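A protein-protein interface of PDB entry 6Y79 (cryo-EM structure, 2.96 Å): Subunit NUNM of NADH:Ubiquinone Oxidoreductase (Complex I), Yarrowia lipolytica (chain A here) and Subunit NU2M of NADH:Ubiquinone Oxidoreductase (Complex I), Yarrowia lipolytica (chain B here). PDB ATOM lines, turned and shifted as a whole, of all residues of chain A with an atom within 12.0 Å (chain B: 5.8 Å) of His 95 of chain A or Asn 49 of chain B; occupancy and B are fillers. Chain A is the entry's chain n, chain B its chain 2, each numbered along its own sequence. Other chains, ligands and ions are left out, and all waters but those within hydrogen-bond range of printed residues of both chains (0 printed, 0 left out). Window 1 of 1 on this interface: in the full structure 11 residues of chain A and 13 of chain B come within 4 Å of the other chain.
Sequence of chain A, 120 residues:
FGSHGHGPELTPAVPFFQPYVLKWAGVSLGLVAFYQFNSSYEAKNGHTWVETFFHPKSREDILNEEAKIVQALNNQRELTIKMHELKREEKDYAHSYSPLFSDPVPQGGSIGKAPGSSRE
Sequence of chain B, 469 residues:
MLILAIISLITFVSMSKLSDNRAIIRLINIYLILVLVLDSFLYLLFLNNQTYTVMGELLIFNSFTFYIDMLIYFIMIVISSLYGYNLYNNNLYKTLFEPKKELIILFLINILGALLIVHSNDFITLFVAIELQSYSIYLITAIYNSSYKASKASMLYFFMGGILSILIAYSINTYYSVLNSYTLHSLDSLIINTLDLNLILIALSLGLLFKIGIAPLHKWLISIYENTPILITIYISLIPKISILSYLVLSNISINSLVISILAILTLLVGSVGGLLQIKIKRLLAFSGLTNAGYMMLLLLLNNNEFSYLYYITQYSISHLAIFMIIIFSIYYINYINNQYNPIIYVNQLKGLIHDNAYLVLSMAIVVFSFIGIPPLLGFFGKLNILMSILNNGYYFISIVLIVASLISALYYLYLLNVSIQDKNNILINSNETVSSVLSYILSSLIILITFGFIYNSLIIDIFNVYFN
Asn 469 of chain B touches Met 83 of chain A (ND2 to CE, 3.4 Å). Lys 87 of chain A touches Asn 469 of chain B (CG to OD1, 3.3 Å). Asn 49 of chain B touches Lys 91 of chain A. O of His 95 of chain A touches O of Asn 49 of chain B, at 3.8 Å. O of Ser 96 of chain A touches CB of Thr 51 of chain B, at 3.2 Å. Ser 98 of chain A touches Thr 51 of chain B (CA to O, 3.7 Å). Pro 99 of chain A touches Gln 50 of chain B (CG to OE1, 3.3 Å). CD of Pro 99 of chain A touches O of Thr 51 of chain B, at 3.9 Å.
Among the printed residues, 13 pairs touch across the chains. Among the printed residues, no Asp or Glu carboxylate lies within 4 Å of a Lys or Arg side-chain nitrogen of the other chain.
His 84 of chain A touches none of the printed residues of chain B. Of the printed residues of chain B, Ala 94 of chain A touches Gln 50 (3.5 Å). Of the printed residues of chain B, Ser 96 of chain A touches Thr 51. Printed residues of chain B within 4 Å of Ser 98 of chain A: Thr 51 (3.7 Å). Gln 50 of chain B touches just these residues of chain A: Ala 94 (3.5 Å), His 95 (3.4 Å) and Pro 99 (3.3 Å). The nearest residue of chain A that does not touch Asn 49 of chain B is Ser 96 of chain A (5.5 Å). The nearest printed residue of chain B that does not touch Lys 87 of chain A is Phe 468 of chain B (4.7 Å).
The backbone carbonyl oxygen (O) of Ala 94 of chain A lies close to the side-chain amide oxygen (OE1) of Gln 50 of chain B (3.5 Å). O of His 95 of chain A sits close to OE1 of Gln 50 of chain B (3.4 Å). The backbone carbonyl oxygen (O) of His 95 of chain A is in hydrogen-bond range of the backbone NH (N) of Thr 51 of chain B. NZ of Lys 91 of chain A is in hydrogen-bond range of O of Asn 48 of chain B (3.1 Å). The backbone carbonyl oxygen (O) of Tyr 97 of chain A lies close to the backbone carbonyl oxygen (O) of Thr 51 of chain B (3.1 Å).
N of Asn 48 of chain B lies within hydrogen-bond range of O of Val 466 of chain B (3.3 Å). The backbone carbonyl oxygen of Phe 468 of chain B sits at hydrogen-bond distance from the side-chain amide nitrogen of Asn 49 of chain B (3.1 Å). N of Asn 49 of chain B is in hydrogen-bond range of O of Tyr 467 of chain B (3.3 Å). The backbone carbonyl oxygen of Asp 92 of chain A sits at hydrogen-bond distance from the side-chain hydroxyl of Ser 96 of chain A, at 3.0 Å. The backbone carbonyl oxygen (O) of Pro 99 of chain A sits at hydrogen-bond distance from the side-chain hydroxyl (OG) of Ser 102 of chain A, at 2.5 Å. The backbone carbonyl oxygen (O) of Leu 100 of chain A is in hydrogen-bond range of the side-chain hydroxyl (OG) of Ser 98 of chain A (3.3 Å).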
ATOM      1  N   MET A  83      -8.408 -16.207  27.861  1.00  0.00           N
ATOM      2  CA  MET A  83      -9.599 -15.377  27.711  1.00  0.00           C
ATOM      3  C   MET A  83      -9.312 -13.895  27.925  1.00  0.00           C
ATOM      4  O   MET A  83     -10.093 -13.059  27.463  1.00  0.00           O
ATOM      5  CB  MET A  83     -10.695 -15.836  28.648  1.00  0.00           C
ATOM      6  CG  MET A  83     -11.186 -17.262  28.434  1.00  0.00           C
ATOM      7  SD  MET A  83     -11.539 -17.661  26.718  1.00  0.00           S
ATOM      8  CE  MET A  83     -13.049 -16.756  26.467  1.00  0.00           C
ATOM      9  N   HIS A  84      -8.217 -13.546  28.608  1.00  0.00           N
ATOM     10  CA  HIS A  84      -7.757 -12.163  28.585  1.00  0.00           C
ATOM     11  C   HIS A  84      -7.099 -11.796  27.261  1.00  0.00           C
ATOM     12  O   HIS A  84      -7.274 -10.664  26.805  1.00  0.00           O
ATOM     13  CB  HIS A  84      -6.782 -11.888  29.728  1.00  0.00           C
ATOM     14  CG  HIS A  84      -7.426 -11.803  31.077  1.00  0.00           C
ATOM     15  ND1 HIS A  84      -8.595 -11.111  31.306  1.00  0.00           N
ATOM     16  CD2 HIS A  84      -7.056 -12.319  32.271  1.00  0.00           C
ATOM     17  CE1 HIS A  84      -8.924 -11.215  32.582  1.00  0.00           C
ATOM     18  NE2 HIS A  84      -8.006 -11.945  33.188  1.00  0.00           N
ATOM     19  N   GLU A  85      -6.316 -12.708  26.658  1.00  0.00           N
ATOM     20  CA  GLU A  85      -5.739 -12.449  25.331  1.00  0.00           C
ATOM     21  C   GLU A  85      -6.820 -12.229  24.281  1.00  0.00           C
ATOM     22  O   GLU A  85      -6.663 -11.410  23.371  1.00  0.00           O
ATOM     23  CB  GLU A  85      -4.898 -13.630  24.859  1.00  0.00           C
ATOM     24  CG  GLU A  85      -3.531 -13.856  25.423  1.00  0.00           C
ATOM     25  CD  GLU A  85      -2.985 -15.194  24.926  1.00  0.00           C
ATOM     26  OE1 GLU A  85      -2.896 -15.374  23.692  1.00  0.00           O
ATOM     27  OE2 GLU A  85      -2.663 -16.070  25.757  1.00  0.00           O
ATOM     28  N   LEU A  86      -7.899 -13.001  24.370  1.00  0.00           N
ATOM     29  CA  LEU A  86      -8.918 -13.036  23.326  1.00  0.00           C
ATOM     30  C   LEU A  86      -9.703 -11.744  23.192  1.00  0.00           C
ATOM     31  O   LEU A  86     -10.245 -11.479  22.115  1.00  0.00           O
ATOM     32  CB  LEU A  86      -9.901 -14.170  23.580  1.00  0.00           C
ATOM     33  CG  LEU A  86      -9.757 -15.513  22.857  1.00  0.00           C
ATOM     34  CD1 LEU A  86      -8.419 -16.224  23.265  1.00  0.00           C
ATOM     35  CD2 LEU A  86     -10.986 -16.406  23.159  1.00  0.00           C
ATOM     36  N   LYS A  87      -9.802 -10.947  24.249  1.00  0.00           N
ATOM     37  CA  LYS A  87     -10.598  -9.732  24.152  1.00  0.00           C
ATOM     38  C   LYS A  87      -9.807  -8.586  23.549  1.00  0.00           C
ATOM     39  O   LYS A  87     -10.372  -7.758  22.833  1.00  0.00           O
ATOM     40  CB  LYS A  87     -11.120  -9.325  25.518  1.00  0.00           C
ATOM     41  CG  LYS A  87     -12.139 -10.259  26.076  1.00  0.00           C
ATOM     42  CD  LYS A  87     -12.817  -9.655  27.287  1.00  0.00           C
ATOM     43  CE  LYS A  87     -13.814  -8.574  26.886  1.00  0.00           C
ATOM     44  NZ  LYS A  87     -14.663  -8.123  28.032  1.00  0.00           N
ATOM     45  N   ARG A  88      -8.514  -8.500  23.852  1.00  0.00           N
ATOM     46  CA  ARG A  88      -7.670  -7.435  23.331  1.00  0.00           C
ATOM     47  C   ARG A  88      -7.267  -7.679  21.886  1.00  0.00           C
ATOM     48  O   ARG A  88      -6.685  -6.789  21.256  1.00  0.00           O
ATOM     49  CB  ARG A  88      -6.414  -7.271  24.198  1.00  0.00           C
ATOM     50  CG  ARG A  88      -6.564  -6.333  25.401  1.00  0.00           C
ATOM     51  CD  ARG A  88      -7.363  -6.972  26.518  1.00  0.00           C
ATOM     52  NE  ARG A  88      -7.507  -6.146  27.704  1.00  0.00           N
ATOM     53  CZ  ARG A  88      -8.347  -6.436  28.687  1.00  0.00           C
ATOM     54  NH1 ARG A  88      -9.101  -7.519  28.594  1.00  0.00           N
ATOM     55  NH2 ARG A  88      -8.449  -5.644  29.749  1.00  0.00           N
ATOM     56  N   GLU A  89      -7.558  -8.862  21.364  1.00  0.00           N
ATOM     57  CA  GLU A  89      -7.341  -9.160  19.961  1.00  0.00           C
ATOM     58  C   GLU A  89      -8.302  -8.359  19.093  1.00  0.00           C
ATOM     59  O   GLU A  89      -9.487  -8.233  19.415  1.00  0.00           O
ATOM     60  CB  GLU A  89      -7.534 -10.652  19.732  1.00  0.00           C
ATOM     61  CG  GLU A  89      -7.292 -11.097  18.329  1.00  0.00           C
ATOM     62  CD  GLU A  89      -7.417 -12.584  18.173  1.00  0.00           C
ATOM     63  OE1 GLU A  89      -7.651 -13.274  19.186  1.00  0.00           O
ATOM     64  OE2 GLU A  89      -7.287 -13.066  17.031  1.00  0.00           O
ATOM     65  N   GLU A  90      -7.782  -7.815  17.995  1.00  0.00           N
ATOM     66  CA  GLU A  90      -8.589  -7.092  17.026  1.00  0.00           C
ATOM     67  C   GLU A  90      -9.582  -8.033  16.355  1.00  0.00           C
ATOM     68  O   GLU A  90      -9.429  -9.257  16.371  1.00  0.00           O
ATOM     69  CB  GLU A  90      -7.696  -6.439  15.971  1.00  0.00           C
ATOM     70  CG  GLU A  90      -6.918  -5.223  16.462  1.00  0.00           C
ATOM     71  CD  GLU A  90      -7.822  -4.084  16.887  1.00  0.00           C
ATOM     72  OE1 GLU A  90      -8.625  -3.623  16.052  1.00  0.00           O
ATOM     73  OE2 GLU A  90      -7.724  -3.639  18.050  1.00  0.00           O
ATOM     74  N   LYS A  91     -10.616  -7.449  15.760  1.00  0.00           N
ATOM     75  CA  LYS A  91     -11.688  -8.250  15.198  1.00  0.00           C
ATOM     76  C   LYS A  91     -12.182  -7.626  13.898  1.00  0.00           C
ATOM     77  O   LYS A  91     -12.187  -6.403  13.726  1.00  0.00           O
ATOM     78  CB  LYS A  91     -12.840  -8.415  16.203  1.00  0.00           C
ATOM     79  CG  LYS A  91     -13.802  -9.539  15.871  1.00  0.00           C
ATOM     80  CD  LYS A  91     -14.874  -9.737  16.922  1.00  0.00           C
ATOM     81  CE  LYS A  91     -14.496 -10.806  17.908  1.00  0.00           C
ATOM     82  NZ  LYS A  91     -15.670 -11.184  18.725  1.00  0.00           N
ATOM     83  N   ASP A  92     -12.596  -8.516  13.000  1.00  0.00           N
ATOM     84  CA  ASP A  92     -13.155  -8.285  11.680  1.00  0.00           C
ATOM     85  C   ASP A  92     -14.286  -7.258  11.684  1.00  0.00           C
ATOM     86  O   ASP A  92     -14.967  -7.043  12.684  1.00  0.00           O
ATOM     87  CB  ASP A  92     -13.699  -9.611  11.189  1.00  0.00           C
ATOM     88  CG  ASP A  92     -13.616  -9.790   9.712  1.00  0.00           C
ATOM     89  OD1 ASP A  92     -12.693  -9.269   9.055  1.00  0.00           O
ATOM     90  OD2 ASP A  92     -14.495 -10.524   9.212  1.00  0.00           O
ATOM     91  N   TYR A  93     -14.505  -6.644  10.520  1.00  0.00           N
ATOM     92  CA  TYR A  93     -15.663  -5.776  10.338  1.00  0.00           C
ATOM     93  C   TYR A  93     -16.952  -6.577  10.253  1.00  0.00           C
ATOM     94  O   TYR A  93     -18.010  -6.084  10.652  1.00  0.00           O
ATOM     95  CB  TYR A  93     -15.466  -4.935   9.084  1.00  0.00           C
ATOM     96  CG  TYR A  93     -16.558  -3.945   8.750  1.00  0.00           C
ATOM     97  CD1 TYR A  93     -16.581  -2.685   9.320  1.00  0.00           C
ATOM     98  CD2 TYR A  93     -17.543  -4.262   7.827  1.00  0.00           C
ATOM     99  CE1 TYR A  93     -17.561  -1.783   8.995  1.00  0.00           C
ATOM    100  CE2 TYR A  93     -18.523  -3.364   7.498  1.00  0.00           C
ATOM    101  CZ  TYR A  93     -18.522  -2.123   8.080  1.00  0.00           C
ATOM    102  OH  TYR A  93     -19.510  -1.224   7.757  1.00  0.00           O
ATOM    103  N   ALA A  94     -16.890  -7.805   9.738  1.00  0.00           N
ATOM    104  CA  ALA A  94     -18.082  -8.638   9.654  1.00  0.00           C
ATOM    105  C   ALA A  94     -18.498  -9.187  11.004  1.00  0.00           C
ATOM    106  O   ALA A  94     -19.657  -9.564  11.172  1.00  0.00           O
ATOM    107  CB  ALA A  94     -17.859  -9.795   8.684  1.00  0.00           C
ATOM    108  N   HIS A  95     -17.581  -9.263  11.964  1.00  0.00           N
ATOM    109  CA  HIS A  95     -17.950  -9.677  13.311  1.00  0.00           C
ATOM    110  C   HIS A  95     -18.249  -8.486  14.220  1.00  0.00           C
ATOM    111  O   HIS A  95     -19.152  -8.565  15.053  1.00  0.00           O
ATOM    112  CB  HIS A  95     -16.841 -10.525  13.937  1.00  0.00           C
ATOM    113  CG  HIS A  95     -16.578 -11.836  13.252  1.00  0.00           C
ATOM    114  ND1 HIS A  95     -17.192 -13.013  13.627  1.00  0.00           N
ATOM    115  CD2 HIS A  95     -15.717 -12.167  12.260  1.00  0.00           C
ATOM    116  CE1 HIS A  95     -16.731 -14.006  12.889  1.00  0.00           C
ATOM    117  NE2 HIS A  95     -15.843 -13.517  12.044  1.00  0.00           N
ATOM    118  N   SER A  96     -17.516  -7.377  14.079  1.00  0.00           N
ATOM    119  CA  SER A  96     -17.728  -6.222  14.949  1.00  0.00           C
ATOM    120  C   SER A  96     -18.961  -5.432  14.540  1.00  0.00           C
ATOM    121  O   SER A  96     -19.746  -5.009  15.390  1.00  0.00           O
ATOM    122  CB  SER A  96     -16.513  -5.303  14.925  1.00  0.00           C
ATOM    123  OG  SER A  96     -15.367  -5.965  15.406  1.00  0.00           O
ATOM    124  N   TYR A  97     -19.100  -5.147  13.255  1.00  0.00           N
ATOM    125  CA  TYR A  97     -20.280  -4.493  12.718  1.00  0.00           C
ATOM    126  C   TYR A  97     -21.187  -5.622  12.212  1.00  0.00           C
ATOM    127  O   TYR A  97     -20.881  -6.795  12.422  1.00  0.00           O
ATOM    128  CB  TYR A  97     -19.813  -3.436  11.704  1.00  0.00           C
ATOM    129  CG  TYR A  97     -20.867  -2.696  10.905  1.00  0.00           C
ATOM    130  CD1 TYR A  97     -21.464  -1.547  11.393  1.00  0.00           C
ATOM    131  CD2 TYR A  97     -21.255  -3.160   9.647  1.00  0.00           C
ATOM    132  CE1 TYR A  97     -22.432  -0.889  10.656  1.00  0.00           C
ATOM    133  CE2 TYR A  97     -22.218  -2.528   8.916  1.00  0.00           C
ATOM    134  CZ  TYR A  97     -22.804  -1.393   9.413  1.00  0.00           C
ATOM    135  OH  TYR A  97     -23.762  -0.761   8.654  1.00  0.00           O
ATOM    136  N   SER A  98     -22.322  -5.295  11.599  1.00  0.00           N
ATOM    137  CA  SER A  98     -23.262  -6.271  11.061  1.00  0.00           C
ATOM    138  C   SER A  98     -22.612  -7.191  10.028  1.00  0.00           C
ATOM    139  O   SER A  98     -21.785  -6.737   9.224  1.00  0.00           O
ATOM    140  CB  SER A  98     -24.456  -5.565  10.414  1.00  0.00           C
ATOM    141  OG  SER A  98     -25.370  -6.488   9.852  1.00  0.00           O
ATOM    142  N   PRO A  99     -22.957  -8.473  10.028  1.00  0.00           N
ATOM    143  CA  PRO A  99     -22.360  -9.457   9.123  1.00  0.00           C
ATOM    144  C   PRO A  99     -22.709  -9.293   7.660  1.00  0.00           C
ATOM    145  O   PRO A  99     -21.820  -9.245   6.807  1.00  0.00           O
ATOM    146  CB  PRO A  99     -22.944 -10.763   9.650  1.00  0.00           C
ATOM    147  CG  PRO A  99     -23.264 -10.467  11.043  1.00  0.00           C
ATOM    148  CD  PRO A  99     -23.810  -9.127  11.023  1.00  0.00           C
ATOM    149  N   LEU A 100     -24.009  -9.277   7.370  1.00  0.00           N
ATOM    150  CA  LEU A 100     -24.506  -8.832   6.078  1.00  0.00           C
ATOM    151  C   LEU A 100     -24.055  -7.401   5.854  1.00  0.00           C
ATOM    152  O   LEU A 100     -24.013  -6.609   6.801  1.00  0.00           O
ATOM    153  CB  LEU A 100     -26.030  -8.923   6.064  1.00  0.00           C
ATOM    154  CG  LEU A 100     -26.930  -8.865   4.838  1.00  0.00           C
ATOM    155  CD1 LEU A 100     -26.713 -10.078   4.021  1.00  0.00           C
ATOM    156  CD2 LEU A 100     -28.373  -8.803   5.270  1.00  0.00           C
ATOM    157  N   PHE A 101     -23.710  -7.085   4.601  1.00  0.00           N
ATOM    158  CA  PHE A 101     -23.058  -5.835   4.194  1.00  0.00           C
ATOM    159  C   PHE A 101     -21.710  -5.664   4.896  1.00  0.00           C
ATOM    160  O   PHE A 101     -21.494  -4.761   5.702  1.00  0.00           O
ATOM    161  CB  PHE A 101     -23.946  -4.611   4.437  1.00  0.00           C
ATOM    162  CG  PHE A 101     -25.145  -4.584   3.597  1.00  0.00           C
ATOM    163  CD1 PHE A 101     -25.067  -4.084   2.314  1.00  0.00           C
ATOM    164  CD2 PHE A 101     -26.350  -5.065   4.065  1.00  0.00           C
ATOM    165  CE1 PHE A 101     -26.163  -4.054   1.515  1.00  0.00           C
ATOM    166  CE2 PHE A 101     -27.453  -5.038   3.268  1.00  0.00           C
ATOM    167  CZ  PHE A 101     -27.353  -4.517   1.999  1.00  0.00           C
ATOM    168  N   SER A 102     -20.800  -6.564   4.543  1.00  0.00           N
ATOM    169  CA  SER A 102     -19.469  -6.580   5.127  1.00  0.00           C
ATOM    170  C   SER A 102     -18.513  -5.564   4.514  1.00  0.00           C
ATOM    171  O   SER A 102     -17.342  -5.552   4.908  1.00  0.00           O
ATOM    172  CB  SER A 102     -18.867  -7.978   5.004  1.00  0.00           C
ATOM    173  OG  SER A 102     -19.607  -8.910   5.762  1.00  0.00           O
ATOM    174  N   ASP A 103     -18.988  -4.670   3.488  1.00  0.00           N
ATOM    175  CA  ASP A 103     -17.884  -3.773   3.180  1.00  0.00           C
ATOM    176  C   ASP A 103     -18.127  -2.380   3.755  1.00  0.00           C
ATOM    177  O   ASP A 103     -19.258  -1.886   3.759  1.00  0.00           O
ATOM    178  CB  ASP A 103     -17.640  -3.688   1.672  1.00  0.00           C
ATOM    179  CG  ASP A 103     -18.816  -3.136   0.897  1.00  0.00           C
ATOM    180  OD1 ASP A 103     -19.972  -3.276   1.348  1.00  0.00           O
ATOM    181  OD2 ASP A 103     -18.570  -2.547  -0.177  1.00  0.00           O
ATOM    182  N   PRO A 104     -17.079  -1.733   4.271  1.00  0.00           N
ATOM    183  CA  PRO A 104     -17.237  -0.373   4.806  1.00  0.00           C
ATOM    184  C   PRO A 104     -17.447   0.703   3.752  1.00  0.00           C
ATOM    185  O   PRO A 104     -17.668   1.863   4.122  1.00  0.00           O
ATOM    186  CB  PRO A 104     -15.916  -0.138   5.558  1.00  0.00           C
ATOM    187  CG  PRO A 104     -15.368  -1.493   5.812  1.00  0.00           C
ATOM    188  CD  PRO A 104     -15.785  -2.323   4.644  1.00  0.00           C
ATOM    189  N   PHE B  46     -26.308 -13.978  19.839  1.00  0.00           N
ATOM    190  CA  PHE B  46     -25.069 -13.295  20.187  1.00  0.00           C
ATOM    191  C   PHE B  46     -24.019 -14.271  20.709  1.00  0.00           C
ATOM    192  O   PHE B  46     -23.546 -14.169  21.828  1.00  0.00           O
ATOM    193  CB  PHE B  46     -25.366 -12.207  21.203  1.00  0.00           C
ATOM    194  CG  PHE B  46     -26.413 -11.247  20.754  1.00  0.00           C
ATOM    195  CD1 PHE B  46     -26.139 -10.348  19.747  1.00  0.00           C
ATOM    196  CD2 PHE B  46     -27.673 -11.253  21.313  1.00  0.00           C
ATOM    197  CE1 PHE B  46     -27.089  -9.476  19.314  1.00  0.00           C
ATOM    198  CE2 PHE B  46     -28.627 -10.374  20.876  1.00  0.00           C
ATOM    199  CZ  PHE B  46     -28.334  -9.491  19.880  1.00  0.00           C
ATOM    200  N   LEU B  47     -23.633 -15.217  19.867  1.00  0.00           N
ATOM    201  CA  LEU B  47     -22.514 -16.094  20.168  1.00  0.00           C
ATOM    202  C   LEU B  47     -21.218 -15.414  19.766  1.00  0.00           C
ATOM    203  O   LEU B  47     -21.149 -14.783  18.709  1.00  0.00           O
ATOM    204  CB  LEU B  47     -22.633 -17.414  19.414  1.00  0.00           C
ATOM    205  CG  LEU B  47     -23.588 -18.524  19.833  1.00  0.00           C
ATOM    206  CD1 LEU B  47     -23.623 -19.586  18.748  1.00  0.00           C
ATOM    207  CD2 LEU B  47     -23.118 -19.137  21.099  1.00  0.00           C
ATOM    208  N   ASN B  48     -20.201 -15.546  20.623  1.00  0.00           N
ATOM    209  CA  ASN B  48     -18.821 -15.138  20.343  1.00  0.00           C
ATOM    210  C   ASN B  48     -18.699 -13.649  20.052  1.00  0.00           C
ATOM    211  O   ASN B  48     -17.872 -13.247  19.230  1.00  0.00           O
ATOM    212  CB  ASN B  48     -18.217 -15.948  19.193  1.00  0.00           C
ATOM    213  CG  ASN B  48     -18.061 -17.409  19.536  1.00  0.00           C
ATOM    214  OD1 ASN B  48     -17.526 -17.756  20.586  1.00  0.00           O
ATOM    215  ND2 ASN B  48     -18.544 -18.275  18.658  1.00  0.00           N
ATOM    216  N   ASN B  49     -19.524 -12.851  20.737  1.00  0.00           N
ATOM    217  CA  ASN B  49     -19.617 -11.400  20.568  1.00  0.00           C
ATOM    218  C   ASN B  49     -19.927 -11.027  19.122  1.00  0.00           C
ATOM    219  O   ASN B  49     -19.274 -10.174  18.519  1.00  0.00           O
ATOM    220  CB  ASN B  49     -18.357 -10.692  21.064  1.00  0.00           C
ATOM    221  CG  ASN B  49     -18.623  -9.277  21.494  1.00  0.00           C
ATOM    222  OD1 ASN B  49     -19.745  -8.794  21.405  1.00  0.00           O
ATOM    223  ND2 ASN B  49     -17.586  -8.594  21.954  1.00  0.00           N
ATOM    224  N   GLN B  50     -20.930 -11.688  18.556  1.00  0.00           N
ATOM    225  CA  GLN B  50     -21.454 -11.294  17.260  1.00  0.00           C
ATOM    226  C   GLN B  50     -22.364 -10.092  17.451  1.00  0.00           C
ATOM    227  O   GLN B  50     -23.297 -10.135  18.255  1.00  0.00           O
ATOM    228  CB  GLN B  50     -22.203 -12.445  16.600  1.00  0.00           C
ATOM    229  CG  GLN B  50     -22.806 -12.083  15.259  1.00  0.00           C
ATOM    230  CD  GLN B  50     -21.766 -11.717  14.237  1.00  0.00           C
ATOM    231  OE1 GLN B  50     -21.620 -10.556  13.874  1.00  0.00           O
ATOM    232  NE2 GLN B  50     -21.031 -12.708  13.765  1.00  0.00           N
ATOM    233  N   THR B  51     -22.090  -9.025  16.721  1.00  0.00           N
ATOM    234  CA  THR B  51     -22.798  -7.769  16.858  1.00  0.00           C
ATOM    235  C   THR B  51     -23.527  -7.441  15.562  1.00  0.00           C
ATOM    236  O   THR B  51     -22.986  -7.619  14.470  1.00  0.00           O
ATOM    237  CB  THR B  51     -21.812  -6.664  17.218  1.00  0.00           C
ATOM    238  OG1 THR B  51     -21.101  -7.025  18.408  1.00  0.00           O
ATOM    239  CG2 THR B  51     -22.495  -5.370  17.445  1.00  0.00           C
ATOM    240  N   ASN B  62     -25.661  -5.866  20.447  1.00  0.00           N
ATOM    241  CA  ASN B  62     -24.770  -6.917  20.884  1.00  0.00           C
ATOM    242  C   ASN B  62     -25.365  -7.549  22.126  1.00  0.00           C
ATOM    243  O   ASN B  62     -26.513  -7.307  22.486  1.00  0.00           O
ATOM    244  CB  ASN B  62     -23.350  -6.404  21.130  1.00  0.00           C
ATOM    245  CG  ASN B  62     -23.311  -5.111  21.888  1.00  0.00           C
ATOM    246  OD1 ASN B  62     -24.317  -4.638  22.382  1.00  0.00           O
ATOM    247  ND2 ASN B  62     -22.134  -4.529  21.987  1.00  0.00           N
ATOM    248  N   SER B  63     -24.575  -8.389  22.763  1.00  0.00           N
ATOM    249  CA  SER B  63     -25.018  -9.121  23.932  1.00  0.00           C
ATOM    250  C   SER B  63     -24.973  -8.299  25.205  1.00  0.00           C
ATOM    251  O   SER B  63     -25.745  -8.582  26.129  1.00  0.00           O
ATOM    252  CB  SER B  63     -24.154 -10.354  24.051  1.00  0.00           C
ATOM    253  OG  SER B  63     -22.839 -10.006  23.694  1.00  0.00           O
ATOM    254  N   VAL B 466     -18.167 -17.057  26.962  1.00  0.00           N
ATOM    255  CA  VAL B 466     -18.588 -17.492  25.634  1.00  0.00           C
ATOM    256  C   VAL B 466     -19.329 -16.376  24.888  1.00  0.00           C
ATOM    257  O   VAL B 466     -19.128 -16.186  23.682  1.00  0.00           O
ATOM    258  CB  VAL B 466     -19.392 -18.809  25.703  1.00  0.00           C
ATOM    259  CG1 VAL B 466     -20.686 -18.662  26.432  1.00  0.00           C
ATOM    260  CG2 VAL B 466     -19.635 -19.337  24.331  1.00  0.00           C
ATOM    261  N   TYR B 467     -20.187 -15.599  25.565  1.00  0.00           N
ATOM    262  CA  TYR B 467     -21.047 -14.738  24.756  1.00  0.00           C
ATOM    263  C   TYR B 467     -20.459 -13.367  24.499  1.00  0.00           C
ATOM    264  O   TYR B 467     -21.005 -12.615  23.694  1.00  0.00           O
ATOM    265  CB  TYR B 467     -22.413 -14.570  25.391  1.00  0.00           C
ATOM    266  CG  TYR B 467     -23.255 -15.810  25.319  1.00  0.00           C
ATOM    267  CD1 TYR B 467     -23.030 -16.782  24.368  1.00  0.00           C
ATOM    268  CD2 TYR B 467     -24.279 -16.008  26.204  1.00  0.00           C
ATOM    269  CE1 TYR B 467     -23.803 -17.919  24.318  1.00  0.00           C
ATOM    270  CE2 TYR B 467     -25.062 -17.137  26.159  1.00  0.00           C
ATOM    271  CZ  TYR B 467     -24.818 -18.088  25.205  1.00  0.00           C
ATOM    272  OH  TYR B 467     -25.581 -19.228  25.138  1.00  0.00           O
ATOM    273  N   PHE B 468     -19.396 -12.990  25.192  1.00  0.00           N
ATOM    274  CA  PHE B 468     -18.795 -11.685  24.968  1.00  0.00           C
ATOM    275  C   PHE B 468     -17.417 -11.785  24.372  1.00  0.00           C
ATOM    276  O   PHE B 468     -16.847 -10.757  24.006  1.00  0.00           O
ATOM    277  CB  PHE B 468     -18.682 -10.850  26.244  1.00  0.00           C
ATOM    278  CG  PHE B 468     -20.016 -10.456  26.888  1.00  0.00           C
ATOM    279  CD1 PHE B 468     -21.247 -10.808  26.414  1.00  0.00           C
ATOM    280  CD2 PHE B 468     -19.971  -9.624  27.923  1.00  0.00           C
ATOM    281  CE1 PHE B 468     -22.389 -10.434  27.042  1.00  0.00           C
ATOM    282  CE2 PHE B 468     -21.081  -9.216  28.564  1.00  0.00           C
ATOM    283  CZ  PHE B 468     -22.307  -9.618  28.097  1.00  0.00           C
ATOM    284  N   ASN B 469     -16.836 -12.973  24.329  1.00  0.00           N
ATOM    285  CA  ASN B 469     -15.522 -13.150  23.720  1.00  0.00           C
ATOM    286  C   ASN B 469     -15.606 -14.097  22.525  1.00  0.00           C
ATOM    287  O   ASN B 469     -15.913 -15.280  22.678  1.00  0.00           O
ATOM    288  CB  ASN B 469     -14.504 -13.684  24.734  1.00  0.00           C
ATOM    289  CG  ASN B 469     -14.525 -12.925  26.052  1.00  0.00           C
ATOM    290  OD1 ASN B 469     -15.007 -11.803  26.134  1.00  0.00           O
ATOM    291  ND2 ASN B 469     -13.980 -13.537  27.089  1.00  0.00           N
